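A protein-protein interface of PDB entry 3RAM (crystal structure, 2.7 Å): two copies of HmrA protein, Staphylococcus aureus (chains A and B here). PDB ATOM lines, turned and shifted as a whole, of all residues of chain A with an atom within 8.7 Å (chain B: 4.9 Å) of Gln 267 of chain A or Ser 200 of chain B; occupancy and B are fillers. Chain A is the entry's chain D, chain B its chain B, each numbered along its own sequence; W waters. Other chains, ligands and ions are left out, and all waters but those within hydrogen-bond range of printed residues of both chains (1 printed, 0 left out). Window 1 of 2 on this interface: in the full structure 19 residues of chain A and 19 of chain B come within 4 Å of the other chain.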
ATOM      1  N   PHE A 177      10.153  18.474 -34.332  1.00  0.00           N
ATOM      2  CA  PHE A 177       9.050  19.382 -34.053  1.00  0.00           C
ATOM      3  C   PHE A 177       9.185  20.614 -34.899  1.00  0.00           C
ATOM      4  O   PHE A 177      10.280  21.132 -35.067  1.00  0.00           O
ATOM      5  CB  PHE A 177       9.003  19.754 -32.578  1.00  0.00           C
ATOM      6  CG  PHE A 177       8.649  18.590 -31.678  1.00  0.00           C
ATOM      7  CD1 PHE A 177       9.625  17.952 -30.922  1.00  0.00           C
ATOM      8  CD2 PHE A 177       7.348  18.127 -31.613  1.00  0.00           C
ATOM      9  CE1 PHE A 177       9.319  16.881 -30.113  1.00  0.00           C
ATOM     10  CE2 PHE A 177       7.027  17.056 -30.803  1.00  0.00           C
ATOM     11  CZ  PHE A 177       8.020  16.425 -30.046  1.00  0.00           C
ATOM     12  N   LEU A 192       5.302  29.760 -32.094  1.00  0.00           N
ATOM     13  CA  LEU A 192       4.956  28.403 -31.681  1.00  0.00           C
ATOM     14  C   LEU A 192       6.290  27.710 -31.468  1.00  0.00           C
ATOM     15  O   LEU A 192       7.092  27.589 -32.395  1.00  0.00           O
ATOM     16  CB  LEU A 192       4.128  27.686 -32.740  1.00  0.00           C
ATOM     17  CG  LEU A 192       2.713  28.247 -32.941  1.00  0.00           C
ATOM     18  CD1 LEU A 192       2.183  27.760 -34.296  1.00  0.00           C
ATOM     19  CD2 LEU A 192       1.759  27.885 -31.780  1.00  0.00           C
ATOM     20  N   ASN A 193       6.510  27.275 -30.231  1.00  0.00           N
ATOM     21  CA  ASN A 193       7.838  26.936 -29.719  1.00  0.00           C
ATOM     22  C   ASN A 193       8.194  25.466 -29.875  1.00  0.00           C
ATOM     23  O   ASN A 193       7.703  24.617 -29.133  1.00  0.00           O
ATOM     24  CB  ASN A 193       7.906  27.337 -28.241  1.00  0.00           C
ATOM     25  CG  ASN A 193       9.318  27.525 -27.753  1.00  0.00           C
ATOM     26  OD1 ASN A 193      10.229  26.828 -28.195  1.00  0.00           O
ATOM     27  ND2 ASN A 193       9.511  28.474 -26.843  1.00  0.00           N
ATOM     28  N   ASP A 196      10.104  24.131 -26.709  1.00  0.00           N
ATOM     29  CA  ASP A 196       9.180  23.724 -25.644  1.00  0.00           C
ATOM     30  C   ASP A 196       8.591  22.356 -25.977  1.00  0.00           C
ATOM     31  O   ASP A 196       8.483  21.504 -25.100  1.00  0.00           O
ATOM     32  CB  ASP A 196       8.070  24.763 -25.412  1.00  0.00           C
ATOM     33  CG  ASP A 196       8.546  25.987 -24.607  1.00  0.00           C
ATOM     34  OD1 ASP A 196       7.782  26.993 -24.538  1.00  0.00           O
ATOM     35  OD2 ASP A 196       9.668  25.927 -24.033  1.00  0.00           O
ATOM     36  N   ALA A 197       8.256  22.133 -27.245  1.00  0.00           N
ATOM     37  CA  ALA A 197       7.793  20.823 -27.684  1.00  0.00           C
ATOM     38  C   ALA A 197       8.819  19.739 -27.348  1.00  0.00           C
ATOM     39  O   ALA A 197       8.461  18.691 -26.814  1.00  0.00           O
ATOM     40  CB  ALA A 197       7.491  20.820 -29.162  1.00  0.00           C
ATOM     41  N   MET A 198      10.088  19.996 -27.655  1.00  0.00           N
ATOM     42  CA  MET A 198      11.151  19.015 -27.416  1.00  0.00           C
ATOM     43  C   MET A 198      11.340  18.745 -25.929  1.00  0.00           C
ATOM     44  O   MET A 198      11.492  17.596 -25.522  1.00  0.00           O
ATOM     45  CB  MET A 198      12.484  19.476 -28.034  1.00  0.00           C
ATOM     46  CG  MET A 198      13.601  18.430 -27.971  1.00  0.00           C
ATOM     47  SD  MET A 198      13.173  16.720 -28.911  1.00  0.00           S
ATOM     48  CE  MET A 198      13.672  17.242 -30.743  1.00  0.00           C
ATOM     49  N   ILE A 199      11.344  19.802 -25.119  1.00  0.00           N
ATOM     50  CA  ILE A 199      11.480  19.659 -23.666  1.00  0.00           C
ATOM     51  C   ILE A 199      10.334  18.817 -23.119  1.00  0.00           C
ATOM     52  O   ILE A 199      10.522  18.010 -22.227  1.00  0.00           O
ATOM     53  CB  ILE A 199      11.484  21.038 -22.946  1.00  0.00           C
ATOM     54  CG1 ILE A 199      12.753  21.838 -23.303  1.00  0.00           C
ATOM     55  CG2 ILE A 199      11.358  20.863 -21.428  1.00  0.00           C
ATOM     56  CD1 ILE A 199      14.037  21.115 -23.030  1.00  0.00           C
ATOM     57  N   SER A 200       9.147  19.018 -23.669  1.00  0.00           N
ATOM     58  CA  SER A 200       7.949  18.371 -23.164  1.00  0.00           C
ATOM     59  C   SER A 200       7.935  16.880 -23.524  1.00  0.00           C
ATOM     60  O   SER A 200       7.465  16.027 -22.757  1.00  0.00           O
ATOM     61  CB  SER A 200       6.721  19.093 -23.721  1.00  0.00           C
ATOM     62  OG  SER A 200       5.563  18.293 -23.578  1.00  0.00           O
ATOM     63  N   TYR A 201       8.448  16.583 -24.709  1.00  0.00           N
ATOM     64  CA  TYR A 201       8.663  15.219 -25.160  1.00  0.00           C
ATOM     65  C   TYR A 201       9.653  14.516 -24.248  1.00  0.00           C
ATOM     66  O   TYR A 201       9.426  13.374 -23.865  1.00  0.00           O
ATOM     67  CB  TYR A 201       9.169  15.213 -26.612  1.00  0.00           C
ATOM     68  CG  TYR A 201       9.732  13.883 -27.070  1.00  0.00           C
ATOM     69  CD1 TYR A 201      11.110  13.685 -27.172  1.00  0.00           C
ATOM     70  CD2 TYR A 201       8.890  12.813 -27.399  1.00  0.00           C
ATOM     71  CE1 TYR A 201      11.627  12.473 -27.599  1.00  0.00           C
ATOM     72  CE2 TYR A 201       9.410  11.594 -27.820  1.00  0.00           C
ATOM     73  CZ  TYR A 201      10.775  11.436 -27.919  1.00  0.00           C
ATOM     74  OH  TYR A 201      11.292  10.229 -28.326  1.00  0.00           O
ATOM     75  N   ASN A 203      10.501  15.338 -21.032  1.00  0.00           N
ATOM     76  CA  ASN A 203       9.845  15.172 -19.729  1.00  0.00           C
ATOM     77  C   ASN A 203       8.913  13.955 -19.775  1.00  0.00           C
ATOM     78  O   ASN A 203       8.787  13.233 -18.791  1.00  0.00           O
ATOM     79  CB  ASN A 203       9.051  16.436 -19.311  1.00  0.00           C
ATOM     80  CG  ASN A 203       9.938  17.630 -18.990  1.00  0.00           C
ATOM     81  OD1 ASN A 203      11.058  17.484 -18.536  1.00  0.00           O
ATOM     82  ND2 ASN A 203       9.415  18.823 -19.210  1.00  0.00           N
ATOM     83  N   GLY A 204       8.262  13.750 -20.921  1.00  0.00           N
ATOM     84  CA  GLY A 204       7.306  12.656 -21.098  1.00  0.00           C
ATOM     85  C   GLY A 204       7.983  11.298 -21.200  1.00  0.00           C
ATOM     86  O   GLY A 204       7.532  10.324 -20.581  1.00  0.00           O
ATOM     87  N   VAL A 205       9.071  11.227 -21.969  1.00  0.00           N
ATOM     88  CA  VAL A 205       9.871  10.004 -22.034  1.00  0.00           C
ATOM     89  C   VAL A 205      10.405   9.612 -20.643  1.00  0.00           C
ATOM     90  O   VAL A 205      10.436   8.429 -20.307  1.00  0.00           O
ATOM     91  CB  VAL A 205      11.045  10.129 -23.052  1.00  0.00           C
ATOM     92  CG1 VAL A 205      11.972   8.906 -22.986  1.00  0.00           C
ATOM     93  CG2 VAL A 205      10.504  10.330 -24.469  1.00  0.00           C
ATOM     94  N   GLN A 207       9.073  10.098 -17.743  1.00  0.00           N
ATOM     95  CA  GLN A 207       7.926   9.568 -17.011  1.00  0.00           C
ATOM     96  C   GLN A 207       7.548   8.155 -17.452  1.00  0.00           C
ATOM     97  O   GLN A 207       7.149   7.346 -16.615  1.00  0.00           O
ATOM     98  CB  GLN A 207       6.711  10.503 -17.182  1.00  0.00           C
ATOM     99  CG  GLN A 207       6.794  11.808 -16.368  1.00  0.00           C
ATOM    100  CD  GLN A 207       5.660  12.798 -16.654  1.00  0.00           C
ATOM    101  OE1 GLN A 207       4.811  12.596 -17.543  1.00  0.00           O
ATOM    102  NE2 GLN A 207       5.653  13.888 -15.897  1.00  0.00           N
ATOM    103  N   GLN A 259       3.106   8.652 -29.255  1.00  0.00           N
ATOM    104  CA  GLN A 259       2.060   9.409 -28.583  1.00  0.00           C
ATOM    105  C   GLN A 259       2.616  10.476 -27.608  1.00  0.00           C
ATOM    106  O   GLN A 259       2.018  11.537 -27.435  1.00  0.00           O
ATOM    107  CB  GLN A 259       1.126   8.449 -27.868  1.00  0.00           C
ATOM    108  CG  GLN A 259       0.350   7.563 -28.804  1.00  0.00           C
ATOM    109  CD  GLN A 259      -0.528   8.360 -29.737  1.00  0.00           C
ATOM    110  OE1 GLN A 259      -1.409   9.076 -29.293  1.00  0.00           O
ATOM    111  NE2 GLN A 259      -0.276   8.267 -31.022  1.00  0.00           N
ATOM    112  N   ILE A 260       3.761  10.212 -26.984  1.00  0.00           N
ATOM    113  CA  ILE A 260       4.420  11.219 -26.149  1.00  0.00           C
ATOM    114  C   ILE A 260       4.814  12.441 -27.014  1.00  0.00           C
ATOM    115  O   ILE A 260       4.622  13.605 -26.601  1.00  0.00           O
ATOM    116  CB  ILE A 260       5.647  10.614 -25.395  1.00  0.00           C
ATOM    117  CG1 ILE A 260       5.167   9.736 -24.221  1.00  0.00           C
ATOM    118  CG2 ILE A 260       6.589  11.698 -24.923  1.00  0.00           C
ATOM    119  CD1 ILE A 260       6.260   8.884 -23.571  1.00  0.00           C
ATOM    120  N   ALA A 261       5.341  12.173 -28.215  1.00  0.00           N
ATOM    121  CA  ALA A 261       5.695  13.230 -29.169  1.00  0.00           C
ATOM    122  C   ALA A 261       4.429  13.963 -29.633  1.00  0.00           C
ATOM    123  O   ALA A 261       4.357  15.185 -29.589  1.00  0.00           O
ATOM    124  CB  ALA A 261       6.459  12.646 -30.359  1.00  0.00           C
ATOM    125  N   ARG A 262       3.425  13.214 -30.060  1.00  0.00           N
ATOM    126  CA  ARG A 262       2.157  13.802 -30.484  1.00  0.00           C
ATOM    127  C   ARG A 262       1.610  14.750 -29.428  1.00  0.00           C
ATOM    128  O   ARG A 262       1.198  15.862 -29.743  1.00  0.00           O
ATOM    129  CB  ARG A 262       1.126  12.707 -30.736  1.00  0.00           C
ATOM    130  CG  ARG A 262      -0.119  13.175 -31.403  1.00  0.00           C
ATOM    131  CD  ARG A 262      -1.157  12.076 -31.394  1.00  0.00           C
ATOM    132  NE  ARG A 262      -2.504  12.628 -31.564  1.00  0.00           N
ATOM    133  CZ  ARG A 262      -3.617  12.102 -31.052  1.00  0.00           C
ATOM    134  NH1 ARG A 262      -3.577  10.988 -30.323  1.00  0.00           N
ATOM    135  NH2 ARG A 262      -4.786  12.708 -31.260  1.00  0.00           N
ATOM    136  N   GLY A 263       1.591  14.292 -28.179  1.00  0.00           N
ATOM    137  CA  GLY A 263       1.110  15.095 -27.052  1.00  0.00           C
ATOM    138  C   GLY A 263       1.915  16.367 -26.842  1.00  0.00           C
ATOM    139  O   GLY A 263       1.331  17.417 -26.629  1.00  0.00           O
ATOM    140  N   ALA A 264       3.249  16.278 -26.897  1.00  0.00           N
ATOM    141  CA  ALA A 264       4.093  17.472 -26.842  1.00  0.00           C
ATOM    142  C   ALA A 264       3.686  18.471 -27.951  1.00  0.00           C
ATOM    143  O   ALA A 264       3.514  19.672 -27.698  1.00  0.00           O
ATOM    144  CB  ALA A 264       5.576  17.107 -26.933  1.00  0.00           C
ATOM    145  N   ALA A 265       3.496  17.971 -29.165  1.00  0.00           N
ATOM    146  CA  ALA A 265       3.085  18.813 -30.271  1.00  0.00           C
ATOM    147  C   ALA A 265       1.770  19.525 -29.931  1.00  0.00           C
ATOM    148  O   ALA A 265       1.638  20.739 -30.119  1.00  0.00           O
ATOM    149  CB  ALA A 265       2.953  17.976 -31.550  1.00  0.00           C
ATOM    150  N   ILE A 266       0.809  18.768 -29.407  1.00  0.00           N
ATOM    151  CA  ILE A 266      -0.516  19.294 -29.088  1.00  0.00           C
ATOM    152  C   ILE A 266      -0.415  20.381 -28.002  1.00  0.00           C
ATOM    153  O   ILE A 266      -1.007  21.449 -28.140  1.00  0.00           O
ATOM    154  CB  ILE A 266      -1.516  18.153 -28.713  1.00  0.00           C
ATOM    155  CG1 ILE A 266      -1.893  17.334 -29.966  1.00  0.00           C
ATOM    156  CG2 ILE A 266      -2.780  18.713 -28.071  1.00  0.00           C
ATOM    157  CD1 ILE A 266      -2.658  16.054 -29.684  1.00  0.00           C
ATOM    158  N   GLN A 267       0.375  20.138 -26.961  1.00  0.00           N
ATOM    159  CA  GLN A 267       0.575  21.132 -25.878  1.00  0.00           C
ATOM    160  C   GLN A 267       1.119  22.485 -26.386  1.00  0.00           C
ATOM    161  O   GLN A 267       0.688  23.553 -25.942  1.00  0.00           O
ATOM    162  CB  GLN A 267       1.542  20.586 -24.802  1.00  0.00           C
ATOM    163  CG  GLN A 267       1.053  19.363 -24.072  1.00  0.00           C
ATOM    164  CD  GLN A 267       1.801  19.112 -22.792  1.00  0.00           C
ATOM    165  OE1 GLN A 267       3.038  19.165 -22.757  1.00  0.00           O
ATOM    166  NE2 GLN A 267       1.054  18.843 -21.710  1.00  0.00           N
ATOM    167  N   THR A 268       2.075  22.420 -27.306  1.00  0.00           N
ATOM    168  CA  THR A 268       2.831  23.592 -27.725  1.00  0.00           C
ATOM    169  C   THR A 268       2.226  24.242 -28.968  1.00  0.00           C
ATOM    170  O   THR A 268       2.550  25.393 -29.298  1.00  0.00           O
ATOM    171  CB  THR A 268       4.294  23.208 -27.980  1.00  0.00           C
ATOM    172  OG1 THR A 268       4.371  22.276 -29.062  1.00  0.00           O
ATOM    173  CG2 THR A 268       4.893  22.570 -26.745  1.00  0.00           C
ATOM    174  N   GLY A 269       1.330  23.516 -29.641  1.00  0.00           N
ATOM    175  CA  GLY A 269       0.706  24.002 -30.874  1.00  0.00           C
ATOM    176  C   GLY A 269       1.542  23.694 -32.106  1.00  0.00           C
ATOM    177  O   GLY A 269       1.270  24.201 -33.199  1.00  0.00           O
ATOM    178  N   CYS A 270       2.559  22.854 -31.922  1.00  0.00           N
ATOM    179  CA  CYS A 270       3.477  22.504 -32.984  1.00  0.00           C
ATOM    180  C   CYS A 270       2.981  21.310 -33.781  1.00  0.00           C
ATOM    181  O   CYS A 270       2.070  20.574 -33.377  1.00  0.00           O
ATOM    182  CB  CYS A 270       4.857  22.165 -32.413  1.00  0.00           C
ATOM    183  SG  CYS A 270       5.858  23.567 -31.906  1.00  0.00           S
ATOM    184  N   ASP A 271       3.607  21.140 -34.937  1.00  0.00           N
ATOM    185  CA  ASP A 271       3.457  19.955 -35.727  1.00  0.00           C
ATOM    186  C   ASP A 271       4.678  19.088 -35.472  1.00  0.00           C
ATOM    187  O   ASP A 271       5.637  19.535 -34.838  1.00  0.00           O
ATOM    188  CB  ASP A 271       3.347  20.324 -37.183  1.00  0.00           C
ATOM    189  CG  ASP A 271       2.285  19.541 -37.865  1.00  0.00           C
ATOM    190  OD1 ASP A 271       2.281  18.276 -37.704  1.00  0.00           O
ATOM    191  OD2 ASP A 271       1.435  20.203 -38.518  1.00  0.00           O
ATOM    192  N   ASP B 196       1.329  11.592 -13.517  1.00  0.00           N
ATOM    193  CA  ASP B 196       2.257  11.960 -14.592  1.00  0.00           C
ATOM    194  C   ASP B 196       1.546  12.897 -15.542  1.00  0.00           C
ATOM    195  O   ASP B 196       2.163  13.846 -16.025  1.00  0.00           O
ATOM    196  CB  ASP B 196       2.804  10.741 -15.362  1.00  0.00           C
ATOM    197  CG  ASP B 196       3.951  10.041 -14.626  1.00  0.00           C
ATOM    198  OD1 ASP B 196       4.333   8.892 -15.027  1.00  0.00           O
ATOM    199  OD2 ASP B 196       4.470  10.658 -13.644  1.00  0.00           O
ATOM    200  N   ALA B 197       0.257  12.649 -15.794  1.00  0.00           N
ATOM    201  CA  ALA B 197      -0.555  13.555 -16.616  1.00  0.00           C
ATOM    202  C   ALA B 197      -0.567  14.971 -16.014  1.00  0.00           C
ATOM    203  O   ALA B 197      -0.328  15.955 -16.717  1.00  0.00           O
ATOM    204  CB  ALA B 197      -1.978  13.017 -16.782  1.00  0.00           C
ATOM    205  N   MET B 198      -0.814  15.050 -14.709  1.00  0.00           N
ATOM    206  CA  MET B 198      -0.877  16.331 -13.990  1.00  0.00           C
ATOM    207  C   MET B 198       0.451  17.098 -14.010  1.00  0.00           C
ATOM    208  O   MET B 198       0.464  18.308 -14.240  1.00  0.00           O
ATOM    209  CB  MET B 198      -1.310  16.114 -12.534  1.00  0.00           C
ATOM    210  CG  MET B 198      -1.561  17.402 -11.751  1.00  0.00           C
ATOM    211  SD  MET B 198      -3.003  18.516 -12.525  1.00  0.00           S
ATOM    212  CE  MET B 198      -4.562  17.560 -11.765  1.00  0.00           C
ATOM    213  N   ILE B 199       1.553  16.397 -13.749  1.00  0.00           N
ATOM    214  CA  ILE B 199       2.890  16.996 -13.790  1.00  0.00           C
ATOM    215  C   ILE B 199       3.172  17.557 -15.195  1.00  0.00           C
ATOM    216  O   ILE B 199       3.677  18.669 -15.348  1.00  0.00           O
ATOM    217  CB  ILE B 199       3.990  15.951 -13.417  1.00  0.00           C
ATOM    218  CG1 ILE B 199       3.803  15.438 -11.977  1.00  0.00           C
ATOM    219  CG2 ILE B 199       5.387  16.528 -13.615  1.00  0.00           C
ATOM    220  CD1 ILE B 199       3.877  16.487 -10.929  1.00  0.00           C
ATOM    221  N   SER B 200       2.835  16.778 -16.217  1.00  0.00           N
ATOM    222  CA  SER B 200       3.032  17.177 -17.606  1.00  0.00           C
ATOM    223  C   SER B 200       2.173  18.367 -17.997  1.00  0.00           C
ATOM    224  O   SER B 200       2.586  19.180 -18.811  1.00  0.00           O
ATOM    225  CB  SER B 200       2.697  16.013 -18.550  1.00  0.00           C
ATOM    226  OG  SER B 200       2.198  16.512 -19.786  1.00  0.00           O
ATOM    227  N   TYR B 201       0.959  18.424 -17.462  1.00  0.00           N
ATOM    228  CA  TYR B 201       0.063  19.556 -17.677  1.00  0.00           C
ATOM    229  C   TYR B 201       0.684  20.830 -17.069  1.00  0.00           C
ATOM    230  O   TYR B 201       0.718  21.871 -17.708  1.00  0.00           O
ATOM    231  CB  TYR B 201      -1.344  19.245 -17.104  1.00  0.00           C
ATOM    232  CG  TYR B 201      -2.213  20.465 -16.921  1.00  0.00           C
ATOM    233  CD1 TYR B 201      -2.422  21.002 -15.661  1.00  0.00           C
ATOM    234  CD2 TYR B 201      -2.795  21.111 -18.017  1.00  0.00           C
ATOM    235  CE1 TYR B 201      -3.193  22.148 -15.483  1.00  0.00           C
ATOM    236  CE2 TYR B 201      -3.572  22.260 -17.852  1.00  0.00           C
ATOM    237  CZ  TYR B 201      -3.767  22.775 -16.581  1.00  0.00           C
ATOM    238  OH  TYR B 201      -4.523  23.919 -16.386  1.00  0.00           O
ATOM    239  N   PHE B 202       1.189  20.710 -15.837  1.00  0.00           N
ATOM    240  CA  PHE B 202       1.860  21.792 -15.096  1.00  0.00           C
ATOM    241  C   PHE B 202       3.161  22.263 -15.744  1.00  0.00           C
ATOM    242  O   PHE B 202       3.506  23.456 -15.673  1.00  0.00           O
ATOM    243  CB  PHE B 202       2.148  21.358 -13.642  1.00  0.00           C
ATOM    244  CG  PHE B 202       1.117  21.839 -12.644  1.00  0.00           C
ATOM    245  CD1 PHE B 202      -0.121  21.224 -12.545  1.00  0.00           C
ATOM    246  CD2 PHE B 202       1.382  22.910 -11.815  1.00  0.00           C
ATOM    247  CE1 PHE B 202      -1.073  21.676 -11.640  1.00  0.00           C
ATOM    248  CE2 PHE B 202       0.431  23.359 -10.909  1.00  0.00           C
ATOM    249  CZ  PHE B 202      -0.792  22.742 -10.822  1.00  0.00           C
ATOM    250  N   ASN B 203       3.909  21.337 -16.335  1.00  0.00           N
ATOM    251  CA  ASN B 203       5.124  21.716 -17.063  1.00  0.00           C
ATOM    252  C   ASN B 203       4.740  22.554 -18.273  1.00  0.00           C
ATOM    253  O   ASN B 203       5.434  23.521 -18.617  1.00  0.00           O
ATOM    254  CB  ASN B 203       5.939  20.485 -17.494  1.00  0.00           C
ATOM    255  CG  ASN B 203       6.650  19.799 -16.329  1.00  0.00           C
ATOM    256  OD1 ASN B 203       6.955  20.416 -15.310  1.00  0.00           O
ATOM    257  ND2 ASN B 203       6.944  18.516 -16.498  1.00  0.00           N
ATOM    258  N   GLY B 204       3.609  22.186 -18.884  1.00  0.00           N
ATOM    259  CA  GLY B 204       3.106  22.825 -20.095  1.00  0.00           C
ATOM    260  C   GLY B 204       2.599  24.226 -19.837  1.00  0.00           C
ATOM    261  O   GLY B 204       2.843  25.134 -20.640  1.00  0.00           O
ATOM    262  N   GLN B 259      -5.750  22.676 -24.336  1.00  0.00           N
ATOM    263  CA  GLN B 259      -4.928  21.859 -25.213  1.00  0.00           C
ATOM    264  C   GLN B 259      -3.703  21.310 -24.480  1.00  0.00           C
ATOM    265  O   GLN B 259      -3.284  20.184 -24.746  1.00  0.00           O
ATOM    266  CB  GLN B 259      -4.539  22.624 -26.477  1.00  0.00           C
ATOM    267  CG  GLN B 259      -5.696  22.864 -27.448  1.00  0.00           C
ATOM    268  CD  GLN B 259      -6.307  21.578 -27.997  1.00  0.00           C
ATOM    269  OE1 GLN B 259      -5.628  20.782 -28.648  1.00  0.00           O
ATOM    270  NE2 GLN B 259      -7.606  21.382 -27.743  1.00  0.00           N
ATOM    271  N   ILE B 260      -3.148  22.069 -23.539  1.00  0.00           N
ATOM    272  CA  ILE B 260      -2.048  21.558 -22.703  1.00  0.00           C
ATOM    273  C   ILE B 260      -2.517  20.314 -21.892  1.00  0.00           C
ATOM    274  O   ILE B 260      -1.774  19.327 -21.791  1.00  0.00           O
ATOM    275  CB  ILE B 260      -1.444  22.662 -21.788  1.00  0.00           C
ATOM    276  CG1 ILE B 260      -0.799  23.754 -22.648  1.00  0.00           C
ATOM    277  CG2 ILE B 260      -0.409  22.077 -20.874  1.00  0.00           C
ATOM    278  CD1 ILE B 260      -0.496  25.064 -21.942  1.00  0.00           C
ATOM    279  N   GLY B 263      -3.059  17.378 -24.409  1.00  0.00           N
ATOM    280  CA  GLY B 263      -1.727  16.889 -24.714  1.00  0.00           C
ATOM    281  C   GLY B 263      -1.144  16.051 -23.594  1.00  0.00           C
ATOM    282  O   GLY B 263      -0.568  15.002 -23.865  1.00  0.00           O
ATOM    283  N   ALA B 264      -1.293  16.506 -22.342  1.00  0.00           N
ATOM    284  CA  ALA B 264      -0.822  15.749 -21.166  1.00  0.00           C
ATOM    285  C   ALA B 264      -1.522  14.404 -21.087  1.00  0.00           C
ATOM    286  O   ALA B 264      -0.886  13.389 -20.783  1.00  0.00           O
ATOM    287  CB  ALA B 264      -1.026  16.529 -19.875  1.00  0.00           C
ATOM    288  N   GLN B 267      -0.019  12.124 -23.902  1.00  0.00           N
ATOM    289  CA  GLN B 267       1.290  11.667 -23.474  1.00  0.00           C
ATOM    290  C   GLN B 267       1.223  10.423 -22.583  1.00  0.00           C
ATOM    291  O   GLN B 267       2.012   9.497 -22.759  1.00  0.00           O
ATOM    292  CB  GLN B 267       2.032  12.801 -22.733  1.00  0.00           C
ATOM    293  CG  GLN B 267       2.518  13.925 -23.639  1.00  0.00           C
ATOM    294  CD  GLN B 267       3.726  14.654 -23.098  1.00  0.00           C
ATOM    295  OE1 GLN B 267       3.799  14.975 -21.907  1.00  0.00           O
ATOM    296  NE2 GLN B 267       4.677  14.943 -23.978  1.00  0.00           N
HETATM  297  O   HOH W   1      -3.033  22.114 -30.175  1.00  0.00           O
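Water W1 bridges the backbone carbonyl oxygen (O) of Ile 266 of chain A (2.9 Å) and the side-chain amide oxygen (OE1) of Gln 259 of chain B (3.3 Å).
Asn 203 of chain A touches Asn 203 of chain B (ND2 to ND2, 3.7 Å).
Gln 207 of chain A touches Ile 199 of chain B (NE2 to CG2, 3.5 Å).
Gly 263 of chain A touches Gly 263 of chain B.
CG of Gln 267 of chain B touches CA of Gly 263 of chain A, 3.9 Å away.
Ala 264 of chain A touches Gln 267 of chain B (N to NE2, 3.5 Å).
CG2 of Ile 266 of chain A touches OE1 of Gln 259 of chain B, 3.6 Å away.
Ile 266 of chain A touches Gly 263 of chain B.
Gln 267 of chain A touches Gly 263 of chain B.
Printed residues of chain A that touch a printed residue of chain B: Ser 200, Asn 203, Gln 207, Ile 260, Gly 263, Ala 264, Ile 266 and Gln 267.
Of the 14 printed residues of chain B, 9 touch a printed residue of chain A.
Printed residues of chain B that touch a printed residue of chain A: Asp 196, Ile 199, Ser 200, Asn 203, Gln 259, Ile 260, Gly 263, Ala 264 and Gln 267.
Hydrophobic or aromatic side chains of chain B within 4 Å of the printed part of chain A: Ile 199, Ile 260 and Ala 264.
Among the printed residues, 14 pairs touch across the chains.
Among the printed residues, no Asp or Glu carboxylate lies within 4 Å of a Lys or Arg side-chain nitrogen of the other chain.
The side-chain amide nitrogen of Asn 203 of chain B sits close to the backbone carbonyl oxygen of Ile 199 of chain B (3.5 Å).
The side-chain hydroxyl (OG1) of Thr 268 of chain A is in hydrogen-bond range of the backbone carbonyl oxygen (O) of Ala 264 of chain A (3.1 Å).
The side-chain hydroxyl (OG) of Ser 200 of chain B is in hydrogen-bond range of the side-chain amide oxygen (OE1) of Gln 267 of chain B (3.1 Å).
The backbone carbonyl oxygen (O) of Ile 199 of chain A lies close to the side-chain amide nitrogen (ND2) of Asn 203 of chain A, 3.3 Å away.
The side-chain hydroxyl (OG) of Ser 200 of chain B is in hydrogen-bond range of the side-chain amide nitrogen (NE2) of Gln 267 of chain A (3.2 Å).
NE2 of Gln 267 of chain B sits at hydrogen-bond distance from O of Ser 200 of chain A (3.2 Å).
The backbone NH (N) of Ala 264 of chain B sits close to the side-chain amide nitrogen (NE2) of Gln 267 of chain A, 3.4 Å away.
The side-chain amide nitrogen of Gln 267 of chain B is in hydrogen-bond range of the backbone carbonyl oxygen of Ile 260 of chain A (2.9 Å).
O of Asp 196 of chain B lies close to OE1 of Gln 207 of chain A (3.3 Å).
The backbone carbonyl oxygen (O) of Ile 260 of chain B lies within hydrogen-bond range of the side-chain amide nitrogen (NE2) of Gln 267 of chain A (2.9 Å).
Ser 200 of chain A touches Gln 267 of chain B, and with the chains exchanged Gln 267 of chain A touches Ser 200 of chain B.
Asn 203 of chain B touches its own counterpart, Asn 203 of chain A.
Gly 263 of chain B touches its own counterpart, Gly 263 of chain A.
Ala 264 of chain A touches Gln 267 of chain B, and with the chains exchanged Gln 267 of chain A touches Ala 264 of chain B.
Positions printed for both chains: 196, 197, 198, 199, 200, 201, 203, 204, 259, 260, 263, 264 and 267.
Gln 267 of chain A touches just these residues of chain B: Ser 200, Ile 260, Gly 263 and Ala 264.
Of chain A, only Gln 267 (3.2 Å) comes within 4 Å of Ser 200 of chain B.
Of chain A, only Gln 267 (2.9 Å) comes within 4 Å of Ile 260 of chain B.
Of the printed residues of chain A, Gln 259 of chain B touches Ile 266.
Of the printed residues of chain B, Gly 263 of chain A touches Gly 263 and Gln 267.
Printed residues of chain A within 4 Å of Gly 263 of chain B: Gly 263, Ile 266 and Gln 267.
The nearest residue of chain B that does not touch Gln 267 of chain A is Gln 259 of chain B (4.1 Å).
The nearest residue of chain A that does not touch Ser 200 of chain B is Gln 207 of chain A (4.05 Å).
The nearest printed residue of chain B that does not touch Ile 266 of chain A is Ile 260 of chain B (5.1 Å).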
